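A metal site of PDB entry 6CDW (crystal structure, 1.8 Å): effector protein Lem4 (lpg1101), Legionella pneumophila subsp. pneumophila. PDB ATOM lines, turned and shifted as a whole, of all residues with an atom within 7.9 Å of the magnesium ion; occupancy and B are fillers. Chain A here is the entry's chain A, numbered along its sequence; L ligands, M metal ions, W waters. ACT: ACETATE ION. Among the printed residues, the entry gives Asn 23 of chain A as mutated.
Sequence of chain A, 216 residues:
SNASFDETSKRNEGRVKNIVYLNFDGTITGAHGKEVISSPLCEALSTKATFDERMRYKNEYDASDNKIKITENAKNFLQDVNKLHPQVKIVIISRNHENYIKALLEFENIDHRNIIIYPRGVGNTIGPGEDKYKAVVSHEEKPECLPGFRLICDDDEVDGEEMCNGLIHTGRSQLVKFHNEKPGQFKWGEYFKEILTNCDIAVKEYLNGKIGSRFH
The magnesium ion is bound by OD1 of Asn 23, O of Asp 25, water W1, OD1 of Asp 155, water W2 and OXT of the ligand.
The side-chain amide oxygen (OD1) of Asn 23 sits close to the side-chain hydroxyl (OG1) of Thr 27, at 3.2 Å. NZ of Lys 132 sits close to ND2 of Asn 23. The backbone carbonyl oxygen of Ile 93 is in hydrogen-bond range of the side-chain amide nitrogen of Asn 23, 3.4 Å away. O of Cys 153 sits at hydrogen-bond distance from N of Asn 23. OG1 of Thr 27 is in hydrogen-bond range of N of Asp 155, 3.0 Å away. The backbone NH of Asp 156 sits at hydrogen-bond distance from the side-chain carboxylate of Asp 154 (2.8 Å). OD2 of Asp 154 lies within salt-bridge range of NZ of Lys 132 (3.1 Å).
Asp 154 touches the magnesium ion. Of the 23 residues printed, 4 come within 4 Å of the magnesium ion. The nearest printed residue that does not touch the magnesium ion is Gly 26 (4.3 Å).
Water W1 lies within hydrogen-bond range of OD2 of Asp 155 (2.6 Å), N of Gly 33 (3.1 Å) and NE2 of His 32 (3.4 Å). Water W2 lies within hydrogen-bond range of the side-chain carboxylate (OD1) of Asp 154, the side-chain amino group (NZ) of Lys 132 and the side-chain amide nitrogen (ND2) of Asn 23.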
ATOM      1  N   LEU A  22      18.241 -18.414  -9.337  1.00  0.00           N
ATOM      2  CA  LEU A  22      18.538 -17.152  -8.668  1.00  0.00           C
ATOM      3  C   LEU A  22      19.990 -16.791  -8.950  1.00  0.00           C
ATOM      4  O   LEU A  22      20.895 -17.600  -8.688  1.00  0.00           O
ATOM      5  CB  LEU A  22      18.311 -17.257  -7.157  1.00  0.00           C
ATOM      6  CG  LEU A  22      16.929 -17.748  -6.685  1.00  0.00           C
ATOM      7  CD1 LEU A  22      16.859 -17.889  -5.189  1.00  0.00           C
ATOM      8  CD2 LEU A  22      15.869 -16.792  -7.187  1.00  0.00           C
ATOM      9  N   ASN A  23      20.223 -15.599  -9.479  1.00  0.00           N
ATOM     10  CA  ASN A  23      21.528 -14.975  -9.326  1.00  0.00           C
ATOM     11  C   ASN A  23      21.841 -14.727  -7.839  1.00  0.00           C
ATOM     12  O   ASN A  23      20.935 -14.635  -6.988  1.00  0.00           O
ATOM     13  CB  ASN A  23      21.545 -13.658 -10.116  1.00  0.00           C
ATOM     14  CG  ASN A  23      22.873 -12.993 -10.048  1.00  0.00           C
ATOM     15  OD1 ASN A  23      22.980 -11.847  -9.620  1.00  0.00           O
ATOM     16  ND2 ASN A  23      23.908 -13.703 -10.524  1.00  0.00           N
ATOM     17  N   PHE A  24      23.135 -14.642  -7.500  1.00  0.00           N
ATOM     18  CA  PHE A  24      23.502 -14.408  -6.108  1.00  0.00           C
ATOM     19  C   PHE A  24      23.786 -12.935  -5.834  1.00  0.00           C
ATOM     20  O   PHE A  24      22.963 -12.255  -5.193  1.00  0.00           O
ATOM     21  CB  PHE A  24      24.705 -15.269  -5.663  1.00  0.00           C
ATOM     22  CG  PHE A  24      24.992 -15.189  -4.166  1.00  0.00           C
ATOM     23  CD1 PHE A  24      24.152 -15.835  -3.242  1.00  0.00           C
ATOM     24  CD2 PHE A  24      26.090 -14.477  -3.700  1.00  0.00           C
ATOM     25  CE1 PHE A  24      24.400 -15.740  -1.860  1.00  0.00           C
ATOM     26  CE2 PHE A  24      26.372 -14.378  -2.296  1.00  0.00           C
ATOM     27  CZ  PHE A  24      25.518 -15.011  -1.384  1.00  0.00           C
ATOM     28  N   ASP A  25      24.927 -12.397  -6.317  1.00  0.00           N
ATOM     29  CA  ASP A  25      25.329 -11.031  -5.938  1.00  0.00           C
ATOM     30  C   ASP A  25      24.374 -10.001  -6.523  1.00  0.00           C
ATOM     31  O   ASP A  25      24.183  -9.955  -7.750  1.00  0.00           O
ATOM     32  CB  ASP A  25      26.755 -10.730  -6.388  1.00  0.00           C
ATOM     33  CG  ASP A  25      27.787 -11.663  -5.779  1.00  0.00           C
ATOM     34  OD1 ASP A  25      28.050 -11.562  -4.576  1.00  0.00           O
ATOM     35  OD2 ASP A  25      28.389 -12.459  -6.532  1.00  0.00           O
ATOM     36  N   GLY A  26      23.806  -9.153  -5.676  1.00  0.00           N
ATOM     37  CA  GLY A  26      22.888  -8.124  -6.129  1.00  0.00           C
ATOM     38  C   GLY A  26      21.452  -8.580  -6.274  1.00  0.00           C
ATOM     39  O   GLY A  26      20.567  -7.740  -6.508  1.00  0.00           O
ATOM     40  N   THR A  27      21.202  -9.881  -6.181  1.00  0.00           N
ATOM     41  CA  THR A  27      19.872 -10.443  -6.219  1.00  0.00           C
ATOM     42  C   THR A  27      19.516 -11.000  -4.847  1.00  0.00           C
ATOM     43  O   THR A  27      18.596 -10.504  -4.206  1.00  0.00           O
ATOM     44  CB  THR A  27      19.797 -11.536  -7.302  1.00  0.00           C
ATOM     45  OG1 THR A  27      20.070 -10.934  -8.572  1.00  0.00           O
ATOM     46  CG2 THR A  27      18.415 -12.199  -7.347  1.00  0.00           C
ATOM     47  N   ILE A  28      20.249 -12.013  -4.387  1.00  0.00           N
ATOM     48  CA  ILE A  28      20.079 -12.433  -2.999  1.00  0.00           C
ATOM     49  C   ILE A  28      20.776 -11.457  -2.038  1.00  0.00           C
ATOM     50  O   ILE A  28      20.300 -11.245  -0.920  1.00  0.00           O
ATOM     51  CB  ILE A  28      20.573 -13.879  -2.832  1.00  0.00           C
ATOM     52  CG1 ILE A  28      19.643 -14.832  -3.603  1.00  0.00           C
ATOM     53  CG2 ILE A  28      20.657 -14.323  -1.345  1.00  0.00           C
ATOM     54  CD1 ILE A  28      20.272 -16.201  -3.863  1.00  0.00           C
ATOM     55  N   THR A  29      21.884 -10.808  -2.464  1.00  0.00           N
ATOM     56  CA  THR A  29      22.515  -9.801  -1.627  1.00  0.00           C
ATOM     57  C   THR A  29      22.147  -8.402  -2.113  1.00  0.00           C
ATOM     58  O   THR A  29      21.509  -8.227  -3.156  1.00  0.00           O
ATOM     59  CB  THR A  29      24.040  -9.922  -1.600  1.00  0.00           C
ATOM     60  OG1 THR A  29      24.534  -9.586  -2.876  1.00  0.00           O
ATOM     61  CG2 THR A  29      24.497 -11.336  -1.218  1.00  0.00           C
ATOM     62  N   ALA A  31      24.363  -6.049  -3.141  1.00  0.00           N
ATOM     63  CA  ALA A  31      25.484  -5.409  -3.828  1.00  0.00           C
ATOM     64  C   ALA A  31      25.786  -6.103  -5.139  1.00  0.00           C
ATOM     65  O   ALA A  31      25.820  -7.345  -5.179  1.00  0.00           O
ATOM     66  CB  ALA A  31      26.725  -5.423  -2.943  1.00  0.00           C
ATOM     67  N   HIS A  32      26.008  -5.320  -6.209  1.00  0.00           N
ATOM     68  CA  HIS A  32      26.347  -5.922  -7.506  1.00  0.00           C
ATOM     69  C   HIS A  32      27.632  -6.726  -7.382  1.00  0.00           C
ATOM     70  O   HIS A  32      28.532  -6.394  -6.608  1.00  0.00           O
ATOM     71  CB  HIS A  32      26.500  -4.856  -8.601  1.00  0.00           C
ATOM     72  CG  HIS A  32      26.775  -5.429  -9.969  1.00  0.00           C
ATOM     73  ND1 HIS A  32      28.046  -5.692 -10.438  1.00  0.00           N
ATOM     74  CD2 HIS A  32      25.935  -5.769 -10.982  1.00  0.00           C
ATOM     75  CE1 HIS A  32      27.982  -6.177 -11.667  1.00  0.00           C
ATOM     76  NE2 HIS A  32      26.706  -6.239 -12.018  1.00  0.00           N
ATOM     77  N   GLY A  33      27.691  -7.820  -8.151  1.00  0.00           N
ATOM     78  CA  GLY A  33      28.861  -8.683  -8.109  1.00  0.00           C
ATOM     79  C   GLY A  33      30.190  -7.974  -8.306  1.00  0.00           C
ATOM     80  O   GLY A  33      31.188  -8.299  -7.636  1.00  0.00           O
ATOM     81  N   LYS A  34      30.242  -6.987  -9.208  1.00  0.00           N
ATOM     82  CA  LYS A  34      31.526  -6.387  -9.574  1.00  0.00           C
ATOM     83  C   LYS A  34      32.194  -5.731  -8.378  1.00  0.00           C
ATOM     84  O   LYS A  34      33.423  -5.786  -8.235  1.00  0.00           O
ATOM     85  CB  LYS A  34      31.357  -5.362 -10.706  1.00  0.00           C
ATOM     86  N   ILE A  93      22.989 -19.549  -9.553  1.00  0.00           N
ATOM     87  CA  ILE A  93      23.961 -19.484 -10.647  1.00  0.00           C
ATOM     88  C   ILE A  93      24.735 -18.181 -10.467  1.00  0.00           C
ATOM     89  O   ILE A  93      24.137 -17.105 -10.384  1.00  0.00           O
ATOM     90  CB  ILE A  93      23.280 -19.545 -12.032  1.00  0.00           C
ATOM     91  CG1 ILE A  93      22.417 -20.814 -12.137  1.00  0.00           C
ATOM     92  CG2 ILE A  93      24.341 -19.463 -13.186  1.00  0.00           C
ATOM     93  CD1 ILE A  93      21.548 -20.913 -13.454  1.00  0.00           C
ATOM     94  N   SER A  94      26.060 -18.279 -10.398  1.00  0.00           N
ATOM     95  CA  SER A  94      26.818 -17.097  -9.978  1.00  0.00           C
ATOM     96  C   SER A  94      28.258 -17.178 -10.464  1.00  0.00           C
ATOM     97  O   SER A  94      28.822 -18.267 -10.555  1.00  0.00           O
ATOM     98  CB  SER A  94      26.738 -16.990  -8.433  1.00  0.00           C
ATOM     99  OG  SER A  94      27.644 -15.984  -7.913  1.00  0.00           O
ATOM    100  N   ARG A  95      28.867 -16.002 -10.785  1.00  0.00           N
ATOM    101  CA  ARG A  95      30.297 -15.882 -11.066  1.00  0.00           C
ATOM    102  C   ARG A  95      31.158 -15.847  -9.802  1.00  0.00           C
ATOM    103  O   ARG A  95      32.396 -15.764  -9.915  1.00  0.00           O
ATOM    104  CB  ARG A  95      30.585 -14.595 -11.868  1.00  0.00           C
ATOM    105  CG  ARG A  95      30.257 -14.661 -13.327  1.00  0.00           C
ATOM    106  CD  ARG A  95      30.532 -13.304 -14.031  1.00  0.00           C
ATOM    107  NE  ARG A  95      29.550 -12.293 -13.627  1.00  0.00           N
ATOM    108  CZ  ARG A  95      28.401 -12.075 -14.278  1.00  0.00           C
ATOM    109  NH1 ARG A  95      28.108 -12.768 -15.380  1.00  0.00           N
ATOM    110  NH2 ARG A  95      27.557 -11.144 -13.826  1.00  0.00           N
ATOM    111  N   LYS A 132      26.002 -18.330 -17.827  1.00  0.00           N
ATOM    112  CA  LYS A 132      24.669 -18.533 -17.260  1.00  0.00           C
ATOM    113  C   LYS A 132      23.751 -19.251 -18.255  1.00  0.00           C
ATOM    114  O   LYS A 132      22.930 -20.108 -17.860  1.00  0.00           O
ATOM    115  CB  LYS A 132      24.082 -17.186 -16.860  1.00  0.00           C
ATOM    116  CG  LYS A 132      24.658 -16.670 -15.507  1.00  0.00           C
ATOM    117  CD  LYS A 132      24.167 -15.263 -15.173  1.00  0.00           C
ATOM    118  CE  LYS A 132      24.705 -14.755 -13.775  1.00  0.00           C
ATOM    119  NZ  LYS A 132      24.549 -13.264 -13.650  1.00  0.00           N
ATOM    120  N   CYS A 153      15.371 -14.821 -11.360  1.00  0.00           N
ATOM    121  CA  CYS A 153      15.662 -13.486 -10.823  1.00  0.00           C
ATOM    122  C   CYS A 153      17.134 -13.124 -11.034  1.00  0.00           C
ATOM    123  O   CYS A 153      18.020 -13.903 -10.659  1.00  0.00           O
ATOM    124  CB  CYS A 153      15.325 -13.421  -9.311  1.00  0.00           C
ATOM    125  SG  CYS A 153      13.571 -13.744  -8.990  1.00  0.00           S
ATOM    126  N   ASP A 154      17.385 -11.940 -11.619  1.00  0.00           N
ATOM    127  CA  ASP A 154      18.755 -11.450 -11.816  1.00  0.00           C
ATOM    128  C   ASP A 154      18.753  -9.940 -11.800  1.00  0.00           C
ATOM    129  O   ASP A 154      17.896  -9.306 -12.425  1.00  0.00           O
ATOM    130  CB  ASP A 154      19.349 -11.971 -13.138  1.00  0.00           C
ATOM    131  CG  ASP A 154      20.891 -11.998 -13.136  1.00  0.00           C
ATOM    132  OD1 ASP A 154      21.533 -11.003 -12.732  1.00  0.00           O
ATOM    133  OD2 ASP A 154      21.454 -13.030 -13.561  1.00  0.00           O
ATOM    134  N   ASP A 155      19.715  -9.336 -11.090  1.00  0.00           N
ATOM    135  CA  ASP A 155      19.800  -7.889 -11.085  1.00  0.00           C
ATOM    136  C   ASP A 155      20.491  -7.341 -12.329  1.00  0.00           C
ATOM    137  O   ASP A 155      20.430  -6.131 -12.586  1.00  0.00           O
ATOM    138  CB  ASP A 155      20.536  -7.436  -9.835  1.00  0.00           C
ATOM    139  CG  ASP A 155      21.977  -7.907  -9.819  1.00  0.00           C
ATOM    140  OD1 ASP A 155      22.181  -9.128  -9.876  1.00  0.00           O
ATOM    141  OD2 ASP A 155      22.900  -7.056  -9.782  1.00  0.00           O
ATOM    142  N   ASP A 156      21.157  -8.205 -13.096  1.00  0.00           N
ATOM    143  CA  ASP A 156      21.780  -7.849 -14.367  1.00  0.00           C
ATOM    144  C   ASP A 156      20.810  -8.286 -15.467  1.00  0.00           C
ATOM    145  O   ASP A 156      20.627  -9.493 -15.705  1.00  0.00           O
ATOM    146  CB  ASP A 156      23.151  -8.516 -14.474  1.00  0.00           C
ATOM    147  CG  ASP A 156      23.919  -8.087 -15.718  1.00  0.00           C
ATOM    148  OD1 ASP A 156      23.311  -7.946 -16.800  1.00  0.00           O
ATOM    149  OD2 ASP A 156      25.153  -7.905 -15.593  1.00  0.00           O
ATOM    150  N   ASP A 159      22.185 -10.718 -18.139  1.00  0.00           N
ATOM    151  CA  ASP A 159      22.398 -12.081 -17.661  1.00  0.00           C
ATOM    152  C   ASP A 159      21.072 -12.779 -17.414  1.00  0.00           C
ATOM    153  O   ASP A 159      20.964 -14.002 -17.621  1.00  0.00           O
ATOM    154  CB  ASP A 159      23.216 -12.060 -16.371  1.00  0.00           C
ATOM    155  CG  ASP A 159      24.646 -11.570 -16.604  1.00  0.00           C
ATOM    156  OD1 ASP A 159      25.006 -11.210 -17.747  1.00  0.00           O
ATOM    157  OD2 ASP A 159      25.410 -11.590 -15.623  1.00  0.00           O
ATOM    158  N   PRO A 183      19.277  -4.061  -7.026  1.00  0.00           N
ATOM    159  CA  PRO A 183      19.482  -4.736  -5.740  1.00  0.00           C
ATOM    160  C   PRO A 183      18.658  -4.073  -4.659  1.00  0.00           C
ATOM    161  O   PRO A 183      18.557  -2.841  -4.610  1.00  0.00           O
ATOM    162  CB  PRO A 183      20.988  -4.585  -5.486  1.00  0.00           C
ATOM    163  CG  PRO A 183      21.588  -4.404  -6.886  1.00  0.00           C
ATOM    164  CD  PRO A 183      20.549  -3.667  -7.676  1.00  0.00           C
ATOM    165  N   PHE A 186      13.762  -6.333  -5.102  1.00  0.00           N
ATOM    166  CA  PHE A 186      13.078  -7.542  -5.564  1.00  0.00           C
ATOM    167  C   PHE A 186      11.853  -7.791  -4.693  1.00  0.00           C
ATOM    168  O   PHE A 186      11.878  -7.537  -3.485  1.00  0.00           O
ATOM    169  CB  PHE A 186      14.032  -8.720  -5.492  1.00  0.00           C
ATOM    170  CG  PHE A 186      15.033  -8.736  -6.609  1.00  0.00           C
ATOM    171  CD1 PHE A 186      16.269  -8.115  -6.471  1.00  0.00           C
ATOM    172  CD2 PHE A 186      14.711  -9.344  -7.820  1.00  0.00           C
ATOM    173  CE1 PHE A 186      17.188  -8.129  -7.515  1.00  0.00           C
ATOM    174  CE2 PHE A 186      15.615  -9.368  -8.856  1.00  0.00           C
ATOM    175  CZ  PHE A 186      16.848  -8.760  -8.713  1.00  0.00           C
HETATM  176  C   ACT L   1      26.584 -12.779  -9.757  1.00  0.00           C
HETATM  177  O   ACT L   1      26.468 -13.479  -8.644  1.00  0.00           O
HETATM  178  OXT ACT L   1      26.294 -11.510  -9.707  1.00  0.00           O
HETATM  179  CH3 ACT L   1      26.984 -13.406 -11.093  1.00  0.00           C
HETATM  180 MG    MG M   1      24.105 -10.177  -9.823  1.00  0.00          MG
HETATM  181  O   HOH W   1      25.143  -8.341  -9.922  1.00  0.00           O
HETATM  182  O   HOH W   2      24.094 -10.590 -11.990  1.00  0.00           O
